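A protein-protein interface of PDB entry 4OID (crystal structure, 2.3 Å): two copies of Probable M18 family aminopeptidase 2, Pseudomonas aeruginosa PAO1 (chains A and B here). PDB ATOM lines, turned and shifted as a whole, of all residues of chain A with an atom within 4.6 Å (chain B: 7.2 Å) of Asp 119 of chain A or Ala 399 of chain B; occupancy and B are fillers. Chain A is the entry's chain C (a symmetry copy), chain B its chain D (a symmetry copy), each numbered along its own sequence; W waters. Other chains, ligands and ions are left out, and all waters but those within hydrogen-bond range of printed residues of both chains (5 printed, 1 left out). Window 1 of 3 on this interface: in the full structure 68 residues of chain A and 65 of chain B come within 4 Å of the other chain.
NH2 of Arg 120 of chain B is in hydrogen-bond range of O of Phe 118 of chain A, at 3.4 Å.
The guanidinium group (NH2) of Arg 120 of chain B is in hydrogen-bond range of the backbone carbonyl oxygen (O) of Asp 119 of chain A, 2.9 Å away.
OG of Ser 402 of chain B lies within hydrogen-bond range of OD2 of Asp 119 of chain A, at 2.8 Å.
The side-chain carboxylate (OD2) of Asp 121 of chain A is in salt-bridge range of the guanidinium group (NH2) of Arg 404 of chain B, at 3.0 Å.
The backbone carbonyl oxygen (O) of Pro 151 of chain A is in hydrogen-bond range of a ring nitrogen (NE2) of His 313 of chain B (2.7 Å).
The backbone carbonyl oxygen (O) of Asn 152 of chain A sits close to the backbone NH (N) of Ala 399 of chain B (3.3 Å).
O of Ile 150 of chain A is in hydrogen-bond range of N of Asp 119 of chain A.
OD2 of Asp 119 of chain A is in hydrogen-bond range of ND2 of Asn 152 of chain A, at 2.5 Å.
The backbone carbonyl oxygen (O) of Pro 116 of chain B is in hydrogen-bond range of the guanidinium group (NE) of Arg 120 of chain B (2.8 Å).
OD1 of Asp 216 of chain B is in hydrogen-bond range of N of Gln 218 of chain B.
N of Phe 398 of chain B is in hydrogen-bond range of O of Leu 406 of chain B (2.9 Å).
The side-chain hydroxyl (OG) of Ser 402 of chain B lies within hydrogen-bond range of the backbone NH (N) of Arg 404 of chain B, 3.0 Å away.
Among the printed residues, merely in contact across the chains: Asp 119 of chain A with Ala 399 of chain B (3.4 Å), Asp 119 of chain A with Arg 404 of chain B (3.5 Å), Arg 120 of chain A with Arg 120 of chain B (3.5 Å), Asp 121 of chain A with Gln 218 of chain B (3.7 Å), Asp 121 of chain A with Ala 231 of chain B (3.5 Å), Val 149 of chain A with Leu 406 of chain B (3.7 Å), Pro 151 of chain A with Phe 398 of chain B (3.8 Å), Asn 152 of chain A with His 313 of chain B (3.5 Å), Ala 154 of chain A with His 310 of chain B (3.8 Å) and Ala 154 of chain A with Met 400 of chain B (2.9 Å).
Of the printed residues of chain B, Phe 118 of chain A touches Arg 120 (3.4 Å).
Asp 119 of chain A touches just these residues of chain B: Arg 120, Ala 399, Ser 402 and Arg 404.
Of the printed residues of chain B, Asp 121 of chain A touches Gln 218, Ala 231 and Arg 404.
Of the printed residues of chain A, Ala 231 of chain B touches Asp 121 (3.5 Å).
Ala 399 of chain B touches just these residues of chain A: Asp 119 (3.4 Å) and Asn 152 (3.2 Å).
Of the printed residues of chain A, Leu 406 of chain B touches Val 149.
Of the 10 printed residues of chain A, 8 touch a printed residue of chain B.
Printed residues of chain A that touch a printed residue of chain B: Phe 118, Asp 119, Arg 120, Asp 121, Val 149, Pro 151, Asn 152 and Ala 154.
Among the printed residues, 16 pairs touch across the chains.
Among the printed residues, Asp or Glu carboxylates within 4 Å of a Lys or Arg side-chain nitrogen of the other chain: Asp 121 of chain A with Arg 404 of chain B (3.0 Å).
Arg 120 of chain B touches its own counterpart, Arg 120 of chain A.
1 position is printed for both chains.
Water W5 lies within hydrogen-bond range of O of Phe 118 of chain A (2.9 Å) and NH2 of Arg 120 of chain B (3.0 Å).
Water W3 bridges the backbone carbonyl oxygen (O) of Pro 151 of chain A (2.9 Å) and a ring nitrogen (NE2) of His 313 of chain B (3.5 Å).
Water W4 bridges the backbone NH (N) of Asp 121 of chain A (2.9 Å) and the side-chain amide nitrogen (NE2) of Gln 218 of chain B (3.0 Å).
Water W2 bridges the backbone NH of Ala 154 of chain A (3.1 Å) and the backbone NH of Ala 399 of chain B (3.3 Å).
Water W1 lies within hydrogen-bond range of the backbone carbonyl oxygen of Ala 115 of chain B (3.1 Å), the guanidinium group of Arg 120 of chain A (3.3 Å) and the backbone carbonyl oxygen of Pro 116 of chain B (3.4 Å).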
ATOM      1  N   TRP A 117      16.169  16.013  15.519  1.00  0.00           N
ATOM      2  CA  TRP A 117      14.826  16.536  15.603  1.00  0.00           C
ATOM      3  C   TRP A 117      14.373  17.236  14.347  1.00  0.00           C
ATOM      4  O   TRP A 117      13.138  17.458  14.187  1.00  0.00           O
ATOM      5  CB  TRP A 117      14.619  17.478  16.826  1.00  0.00           C
ATOM      6  CG  TRP A 117      14.521  16.719  18.088  1.00  0.00           C
ATOM      7  CD1 TRP A 117      15.548  16.100  18.740  1.00  0.00           C
ATOM      8  CD2 TRP A 117      13.334  16.401  18.817  1.00  0.00           C
ATOM      9  NE1 TRP A 117      15.070  15.455  19.848  1.00  0.00           N
ATOM     10  CE2 TRP A 117      13.712  15.603  19.901  1.00  0.00           C
ATOM     11  CE3 TRP A 117      11.993  16.713  18.655  1.00  0.00           C
ATOM     12  CZ2 TRP A 117      12.789  15.105  20.832  1.00  0.00           C
ATOM     13  CZ3 TRP A 117      11.066  16.185  19.568  1.00  0.00           C
ATOM     14  CH2 TRP A 117      11.474  15.399  20.626  1.00  0.00           C
ATOM     15  N   PHE A 118      15.300  17.563  13.463  1.00  0.00           N
ATOM     16  CA  PHE A 118      14.943  18.241  12.245  1.00  0.00           C
ATOM     17  C   PHE A 118      14.309  17.217  11.251  1.00  0.00           C
ATOM     18  O   PHE A 118      14.577  15.985  11.321  1.00  0.00           O
ATOM     19  CB  PHE A 118      16.143  18.932  11.607  1.00  0.00           C
ATOM     20  CG  PHE A 118      16.602  20.149  12.297  1.00  0.00           C
ATOM     21  CD1 PHE A 118      17.235  20.087  13.488  1.00  0.00           C
ATOM     22  CD2 PHE A 118      16.397  21.385  11.750  1.00  0.00           C
ATOM     23  CE1 PHE A 118      17.669  21.242  14.156  1.00  0.00           C
ATOM     24  CE2 PHE A 118      16.835  22.540  12.387  1.00  0.00           C
ATOM     25  CZ  PHE A 118      17.530  22.457  13.577  1.00  0.00           C
ATOM     26  N   ASP A 119      13.363  17.694  10.432  1.00  0.00           N
ATOM     27  CA  ASP A 119      12.786  16.841   9.380  1.00  0.00           C
ATOM     28  C   ASP A 119      12.082  15.585   9.923  1.00  0.00           C
ATOM     29  O   ASP A 119      12.199  14.472   9.395  1.00  0.00           O
ATOM     30  CB  ASP A 119      13.915  16.485   8.366  1.00  0.00           C
ATOM     31  CG  ASP A 119      14.599  17.750   7.803  1.00  0.00           C
ATOM     32  OD1 ASP A 119      13.868  18.777   7.802  1.00  0.00           O
ATOM     33  OD2 ASP A 119      15.826  17.728   7.419  1.00  0.00           O
ATOM     34  N   ARG A 120      11.307  15.782  10.980  1.00  0.00           N
ATOM     35  CA  ARG A 120      10.482  14.747  11.573  1.00  0.00           C
ATOM     36  C   ARG A 120       9.031  15.193  11.656  1.00  0.00           C
ATOM     37  O   ARG A 120       8.726  16.380  11.936  1.00  0.00           O
ATOM     38  CB  ARG A 120      10.978  14.461  12.978  1.00  0.00           C
ATOM     39  CG  ARG A 120      12.439  14.007  13.120  1.00  0.00           C
ATOM     40  CD  ARG A 120      12.651  12.549  12.750  1.00  0.00           C
ATOM     41  NE  ARG A 120      14.060  12.238  12.841  1.00  0.00           N
ATOM     42  CZ  ARG A 120      14.589  11.016  12.753  1.00  0.00           C
ATOM     43  NH1 ARG A 120      13.844   9.948  12.587  1.00  0.00           N
ATOM     44  NH2 ARG A 120      15.885  10.846  12.930  1.00  0.00           N
ATOM     45  N   ASP A 121       8.132  14.226  11.512  1.00  0.00           N
ATOM     46  CA  ASP A 121       6.708  14.480  11.686  1.00  0.00           C
ATOM     47  C   ASP A 121       6.335  14.497  13.189  1.00  0.00           C
ATOM     48  O   ASP A 121       6.147  13.405  13.789  1.00  0.00           O
ATOM     49  CB  ASP A 121       5.871  13.448  10.978  1.00  0.00           C
ATOM     50  CG  ASP A 121       6.032  13.463   9.462  1.00  0.00           C
ATOM     51  OD1 ASP A 121       6.876  14.203   8.913  1.00  0.00           O
ATOM     52  OD2 ASP A 121       5.339  12.648   8.805  1.00  0.00           O
ATOM     53  N   VAL A 149       6.645  20.559  12.374  1.00  0.00           N
ATOM     54  CA  VAL A 149       7.892  20.099  11.792  1.00  0.00           C
ATOM     55  C   VAL A 149       8.936  21.165  11.959  1.00  0.00           C
ATOM     56  O   VAL A 149       8.609  22.343  12.011  1.00  0.00           O
ATOM     57  CB  VAL A 149       7.734  19.715  10.296  1.00  0.00           C
ATOM     58  CG1 VAL A 149       7.145  20.928   9.595  1.00  0.00           C
ATOM     59  CG2 VAL A 149       9.101  19.361   9.666  1.00  0.00           C
ATOM     60  N   ILE A 150      10.189  20.739  12.140  1.00  0.00           N
ATOM     61  CA  ILE A 150      11.287  21.653  12.244  1.00  0.00           C
ATOM     62  C   ILE A 150      12.199  21.417  11.015  1.00  0.00           C
ATOM     63  O   ILE A 150      13.067  20.527  10.996  1.00  0.00           O
ATOM     64  CB  ILE A 150      12.137  21.410  13.522  1.00  0.00           C
ATOM     65  CG1 ILE A 150      11.323  21.472  14.816  1.00  0.00           C
ATOM     66  CG2 ILE A 150      13.220  22.436  13.657  1.00  0.00           C
ATOM     67  CD1 ILE A 150      12.072  20.759  15.942  1.00  0.00           C
ATOM     68  N   PRO A 151      12.064  22.221  10.012  1.00  0.00           N
ATOM     69  CA  PRO A 151      12.767  21.811   8.806  1.00  0.00           C
ATOM     70  C   PRO A 151      14.218  22.253   8.827  1.00  0.00           C
ATOM     71  O   PRO A 151      14.526  23.284   9.411  1.00  0.00           O
ATOM     72  CB  PRO A 151      11.995  22.542   7.699  1.00  0.00           C
ATOM     73  CG  PRO A 151      10.859  23.204   8.347  1.00  0.00           C
ATOM     74  CD  PRO A 151      11.288  23.431   9.756  1.00  0.00           C
ATOM     75  N   ASN A 152      15.115  21.443   8.273  1.00  0.00           N
ATOM     76  CA  ASN A 152      16.491  21.872   7.989  1.00  0.00           C
ATOM     77  C   ASN A 152      16.525  23.027   6.974  1.00  0.00           C
ATOM     78  O   ASN A 152      15.660  23.137   6.138  1.00  0.00           O
ATOM     79  CB  ASN A 152      17.298  20.720   7.414  1.00  0.00           C
ATOM     80  CG  ASN A 152      18.065  19.958   8.473  1.00  0.00           C
ATOM     81  OD1 ASN A 152      18.809  20.551   9.236  1.00  0.00           O
ATOM     82  ND2 ASN A 152      17.939  18.633   8.470  1.00  0.00           N
ATOM     83  N   ALA A 154      18.118  24.032   3.615  1.00  0.00           N
ATOM     84  CA  ALA A 154      18.632  23.282   2.455  1.00  0.00           C
ATOM     85  C   ALA A 154      20.167  23.364   2.273  1.00  0.00           C
ATOM     86  O   ALA A 154      20.777  24.408   2.619  1.00  0.00           O
ATOM     87  CB  ALA A 154      17.929  23.736   1.179  1.00  0.00           C
ATOM     88  N   LEU B 113      22.358  16.085   2.195  1.00  0.00           N
ATOM     89  CA  LEU B 113      22.623  16.481   3.617  1.00  0.00           C
ATOM     90  C   LEU B 113      22.843  15.182   4.461  1.00  0.00           C
ATOM     91  O   LEU B 113      21.972  14.344   4.530  1.00  0.00           O
ATOM     92  CB  LEU B 113      21.445  17.251   4.215  1.00  0.00           C
ATOM     93  CG  LEU B 113      21.192  18.724   3.889  1.00  0.00           C
ATOM     94  CD1 LEU B 113      19.959  19.244   4.601  1.00  0.00           C
ATOM     95  CD2 LEU B 113      22.393  19.587   4.245  1.00  0.00           C
ATOM     96  N   ALA B 115      23.392  14.499   7.993  1.00  0.00           N
ATOM     97  CA  ALA B 115      22.829  14.372   9.334  1.00  0.00           C
ATOM     98  C   ALA B 115      21.399  13.721   9.390  1.00  0.00           C
ATOM     99  O   ALA B 115      21.161  12.824  10.186  1.00  0.00           O
ATOM    100  CB  ALA B 115      22.848  15.756  10.044  1.00  0.00           C
ATOM    101  N   PRO B 116      20.473  14.153   8.517  1.00  0.00           N
ATOM    102  CA  PRO B 116      19.129  13.623   8.537  1.00  0.00           C
ATOM    103  C   PRO B 116      19.069  12.154   8.221  1.00  0.00           C
ATOM    104  O   PRO B 116      18.116  11.454   8.597  1.00  0.00           O
ATOM    105  CB  PRO B 116      18.421  14.412   7.428  1.00  0.00           C
ATOM    106  CG  PRO B 116      19.428  15.271   6.811  1.00  0.00           C
ATOM    107  CD  PRO B 116      20.543  15.409   7.772  1.00  0.00           C
ATOM    108  N   ARG B 120      17.160   6.640  11.072  1.00  0.00           N
ATOM    109  CA  ARG B 120      16.035   6.500  10.142  1.00  0.00           C
ATOM    110  C   ARG B 120      15.907   5.032   9.858  1.00  0.00           C
ATOM    111  O   ARG B 120      16.941   4.352   9.734  1.00  0.00           O
ATOM    112  CB  ARG B 120      16.345   7.257   8.836  1.00  0.00           C
ATOM    113  CG  ARG B 120      16.435   8.780   8.983  1.00  0.00           C
ATOM    114  CD  ARG B 120      15.113   9.550   9.154  1.00  0.00           C
ATOM    115  NE  ARG B 120      15.406  10.951   9.298  1.00  0.00           N
ATOM    116  CZ  ARG B 120      14.489  11.916   9.339  1.00  0.00           C
ATOM    117  NH1 ARG B 120      13.193  11.625   9.277  1.00  0.00           N
ATOM    118  NH2 ARG B 120      14.850  13.190   9.462  1.00  0.00           N
ATOM    119  N   ASP B 216      14.310   5.862   2.946  1.00  0.00           N
ATOM    120  CA  ASP B 216      13.459   5.828   4.158  1.00  0.00           C
ATOM    121  C   ASP B 216      12.161   5.050   3.990  1.00  0.00           C
ATOM    122  O   ASP B 216      11.405   5.314   3.053  1.00  0.00           O
ATOM    123  CB  ASP B 216      13.104   7.269   4.508  1.00  0.00           C
ATOM    124  CG  ASP B 216      12.624   7.471   5.959  1.00  0.00           C
ATOM    125  OD1 ASP B 216      12.320   6.499   6.694  1.00  0.00           O
ATOM    126  OD2 ASP B 216      12.507   8.666   6.312  1.00  0.00           O
ATOM    127  N   GLN B 218       9.649   5.353   6.113  1.00  0.00           N
ATOM    128  CA  GLN B 218       8.534   6.199   6.490  1.00  0.00           C
ATOM    129  C   GLN B 218       7.892   6.882   5.243  1.00  0.00           C
ATOM    130  O   GLN B 218       8.526   7.661   4.577  1.00  0.00           O
ATOM    131  CB  GLN B 218       8.970   7.243   7.500  1.00  0.00           C
ATOM    132  CG  GLN B 218       7.768   8.095   7.969  1.00  0.00           C
ATOM    133  CD  GLN B 218       8.153   9.200   9.005  1.00  0.00           C
ATOM    134  OE1 GLN B 218       9.246   9.671   9.037  1.00  0.00           O
ATOM    135  NE2 GLN B 218       7.226   9.628   9.766  1.00  0.00           N
ATOM    136  N   ALA B 231       5.219  16.184   3.755  1.00  0.00           N
ATOM    137  CA  ALA B 231       6.591  15.794   4.191  1.00  0.00           C
ATOM    138  C   ALA B 231       6.911  14.488   3.559  1.00  0.00           C
ATOM    139  O   ALA B 231       6.065  13.583   3.611  1.00  0.00           O
ATOM    140  CB  ALA B 231       6.675  15.636   5.723  1.00  0.00           C
ATOM    141  N   GLY B 232       8.136  14.329   3.054  1.00  0.00           N
ATOM    142  CA  GLY B 232       8.541  13.056   2.501  1.00  0.00           C
ATOM    143  C   GLY B 232       9.888  13.094   1.809  1.00  0.00           C
ATOM    144  O   GLY B 232      10.384  14.166   1.459  1.00  0.00           O
ATOM    145  N   HIS B 310      13.520  27.090  -3.063  1.00  0.00           N
ATOM    146  CA  HIS B 310      13.668  27.246  -1.643  1.00  0.00           C
ATOM    147  C   HIS B 310      12.655  28.228  -1.168  1.00  0.00           C
ATOM    148  O   HIS B 310      12.648  29.351  -1.659  1.00  0.00           O
ATOM    149  CB  HIS B 310      15.043  27.773  -1.363  1.00  0.00           C
ATOM    150  CG  HIS B 310      16.108  26.921  -1.944  1.00  0.00           C
ATOM    151  ND1 HIS B 310      16.238  25.590  -1.625  1.00  0.00           N
ATOM    152  CD2 HIS B 310      17.093  27.202  -2.830  1.00  0.00           C
ATOM    153  CE1 HIS B 310      17.265  25.085  -2.289  1.00  0.00           C
ATOM    154  NE2 HIS B 310      17.807  26.044  -3.022  1.00  0.00           N
ATOM    155  N   GLY B 311      11.758  27.800  -0.270  1.00  0.00           N
ATOM    156  CA  GLY B 311      10.807  28.726   0.359  1.00  0.00           C
ATOM    157  C   GLY B 311      11.625  29.518   1.386  1.00  0.00           C
ATOM    158  O   GLY B 311      12.673  29.040   1.837  1.00  0.00           O
ATOM    159  N   HIS B 313      12.653  30.306   4.763  1.00  0.00           N
ATOM    160  CA  HIS B 313      12.589  29.525   6.018  1.00  0.00           C
ATOM    161  C   HIS B 313      12.507  30.521   7.191  1.00  0.00           C
ATOM    162  O   HIS B 313      13.443  31.263   7.395  1.00  0.00           O
ATOM    163  CB  HIS B 313      13.884  28.646   6.129  1.00  0.00           C
ATOM    164  CG  HIS B 313      13.822  27.533   7.136  1.00  0.00           C
ATOM    165  ND1 HIS B 313      13.258  27.678   8.391  1.00  0.00           N
ATOM    166  CD2 HIS B 313      14.284  26.258   7.074  1.00  0.00           C
ATOM    167  CE1 HIS B 313      13.356  26.533   9.050  1.00  0.00           C
ATOM    168  NE2 HIS B 313      13.984  25.657   8.275  1.00  0.00           N
ATOM    169  N   THR B 397       9.995  24.661  -1.265  1.00  0.00           N
ATOM    170  CA  THR B 397      10.345  23.474  -0.576  1.00  0.00           C
ATOM    171  C   THR B 397      11.307  23.909   0.564  1.00  0.00           C
ATOM    172  O   THR B 397      12.164  24.819   0.370  1.00  0.00           O
ATOM    173  CB  THR B 397      11.080  22.588  -1.618  1.00  0.00           C
ATOM    174  OG1 THR B 397      10.105  21.828  -2.351  1.00  0.00           O
ATOM    175  CG2 THR B 397      12.023  21.676  -1.019  1.00  0.00           C
ATOM    176  N   PHE B 398      11.237  23.242   1.708  1.00  0.00           N
ATOM    177  CA  PHE B 398      12.224  23.448   2.731  1.00  0.00           C
ATOM    178  C   PHE B 398      13.041  22.161   2.813  1.00  0.00           C
ATOM    179  O   PHE B 398      12.565  21.103   2.470  1.00  0.00           O
ATOM    180  CB  PHE B 398      11.571  23.691   4.083  1.00  0.00           C
ATOM    181  CG  PHE B 398      10.884  24.996   4.237  1.00  0.00           C
ATOM    182  CD1 PHE B 398      11.403  26.156   3.697  1.00  0.00           C
ATOM    183  CD2 PHE B 398       9.760  25.089   5.062  1.00  0.00           C
ATOM    184  CE1 PHE B 398      10.721  27.377   3.867  1.00  0.00           C
ATOM    185  CE2 PHE B 398       9.103  26.282   5.253  1.00  0.00           C
ATOM    186  CZ  PHE B 398       9.584  27.444   4.667  1.00  0.00           C
ATOM    187  N   ALA B 399      14.233  22.259   3.350  1.00  0.00           N
ATOM    188  CA  ALA B 399      15.022  21.086   3.708  1.00  0.00           C
ATOM    189  C   ALA B 399      15.366  20.264   2.472  1.00  0.00           C
ATOM    190  O   ALA B 399      15.410  19.041   2.539  1.00  0.00           O
ATOM    191  CB  ALA B 399      14.271  20.236   4.788  1.00  0.00           C
ATOM    192  N   MET B 400      15.545  20.945   1.325  1.00  0.00           N
ATOM    193  CA  MET B 400      16.114  20.337   0.088  1.00  0.00           C
ATOM    194  C   MET B 400      17.556  20.004   0.440  1.00  0.00           C
ATOM    195  O   MET B 400      18.333  20.870   0.849  1.00  0.00           O
ATOM    196  CB  MET B 400      16.064  21.395  -1.028  1.00  0.00           C
ATOM    197  CG  MET B 400      15.962  20.845  -2.443  1.00  0.00           C
ATOM    198  SD  MET B 400      16.268  22.082  -3.752  1.00  0.00           S
ATOM    199  CE  MET B 400      14.787  23.065  -3.472  1.00  0.00           C
ATOM    200  N   HIS B 401      18.107  18.845   0.386  1.00  0.00           N
ATOM    201  CA  HIS B 401      17.909  17.609  -0.150  1.00  0.00           C
ATOM    202  C   HIS B 401      18.148  16.754   1.162  1.00  0.00           C
ATOM    203  O   HIS B 401      19.156  16.075   1.303  1.00  0.00           O
ATOM    204  CB  HIS B 401      19.256  17.440  -0.880  1.00  0.00           C
ATOM    205  CG  HIS B 401      19.322  18.020  -2.261  1.00  0.00           C
ATOM    206  ND1 HIS B 401      20.517  18.479  -2.803  1.00  0.00           N
ATOM    207  CD2 HIS B 401      18.401  18.050  -3.266  1.00  0.00           C
ATOM    208  CE1 HIS B 401      20.300  18.820  -4.065  1.00  0.00           C
ATOM    209  NE2 HIS B 401      19.022  18.588  -4.364  1.00  0.00           N
ATOM    210  N   SER B 402      17.342  16.972   2.185  1.00  0.00           N
ATOM    211  CA  SER B 402      17.253  16.092   3.322  1.00  0.00           C
ATOM    212  C   SER B 402      16.677  14.772   2.874  1.00  0.00           C
ATOM    213  O   SER B 402      16.168  14.657   1.793  1.00  0.00           O
ATOM    214  CB  SER B 402      16.282  16.705   4.364  1.00  0.00           C
ATOM    215  OG  SER B 402      16.089  15.808   5.400  1.00  0.00           O
ATOM    216  N   ILE B 403      16.773  13.769   3.712  1.00  0.00           N
ATOM    217  CA  ILE B 403      15.977  12.552   3.545  1.00  0.00           C
ATOM    218  C   ILE B 403      14.424  12.766   3.718  1.00  0.00           C
ATOM    219  O   ILE B 403      13.627  11.880   3.399  1.00  0.00           O
ATOM    220  CB  ILE B 403      16.470  11.511   4.518  1.00  0.00           C
ATOM    221  CG1 ILE B 403      16.059  10.101   4.066  1.00  0.00           C
ATOM    222  CG2 ILE B 403      16.005  11.844   5.937  1.00  0.00           C
ATOM    223  CD1 ILE B 403      16.503   9.012   5.098  1.00  0.00           C
ATOM    224  N   ARG B 404      14.033  13.894   4.291  1.00  0.00           N
ATOM    225  CA  ARG B 404      12.626  14.258   4.424  1.00  0.00           C
ATOM    226  C   ARG B 404      12.421  15.768   4.230  1.00  0.00           C
ATOM    227  O   ARG B 404      12.742  16.574   5.113  1.00  0.00           O
ATOM    228  CB  ARG B 404      12.081  13.839   5.820  1.00  0.00           C
ATOM    229  CG  ARG B 404      10.577  13.771   5.919  1.00  0.00           C
ATOM    230  CD  ARG B 404      10.110  12.825   7.044  1.00  0.00           C
ATOM    231  NE  ARG B 404       8.656  12.604   7.047  1.00  0.00           N
ATOM    232  CZ  ARG B 404       8.047  11.633   6.347  1.00  0.00           C
ATOM    233  NH1 ARG B 404       8.747  10.823   5.532  1.00  0.00           N
ATOM    234  NH2 ARG B 404       6.705  11.474   6.411  1.00  0.00           N
ATOM    235  N   GLU B 405      11.859  16.125   3.095  1.00  0.00           N
ATOM    236  CA  GLU B 405      11.695  17.519   2.659  1.00  0.00           C
ATOM    237  C   GLU B 405      10.284  17.932   3.011  1.00  0.00           C
ATOM    238  O   GLU B 405       9.492  17.084   3.394  1.00  0.00           O
ATOM    239  CB  GLU B 405      11.901  17.618   1.139  1.00  0.00           C
ATOM    240  CG  GLU B 405      13.411  17.439   0.755  1.00  0.00           C
ATOM    241  CD  GLU B 405      13.685  17.024  -0.717  1.00  0.00           C
ATOM    242  OE1 GLU B 405      12.793  16.405  -1.355  1.00  0.00           O
ATOM    243  OE2 GLU B 405      14.823  17.310  -1.230  1.00  0.00           O
ATOM    244  N   LEU B 406      10.007  19.246   2.911  1.00  0.00           N
ATOM    245  CA  LEU B 406       8.701  19.787   3.239  1.00  0.00           C
ATOM    246  C   LEU B 406       8.235  20.660   2.092  1.00  0.00           C
ATOM    247  O   LEU B 406       8.916  21.572   1.743  1.00  0.00           O
ATOM    248  CB  LEU B 406       8.801  20.632   4.499  1.00  0.00           C
ATOM    249  CG  LEU B 406       7.434  20.943   5.112  1.00  0.00           C
ATOM    250  CD1 LEU B 406       6.818  19.682   5.700  1.00  0.00           C
ATOM    251  CD2 LEU B 406       7.570  22.069   6.129  1.00  0.00           C
HETATM  252  O   HOH W   1      18.530  12.419  11.829  1.00  0.00           O
HETATM  253  O   HOH W   2      15.407  25.362   3.176  1.00  0.00           O
HETATM  254  O   HOH W   3      14.360  25.087  11.679  1.00  0.00           O
HETATM  255  O   HOH W   4       8.784  11.379  11.579  1.00  0.00           O
HETATM  256  O   HOH W   5      16.968  14.435  11.110  1.00  0.00           O
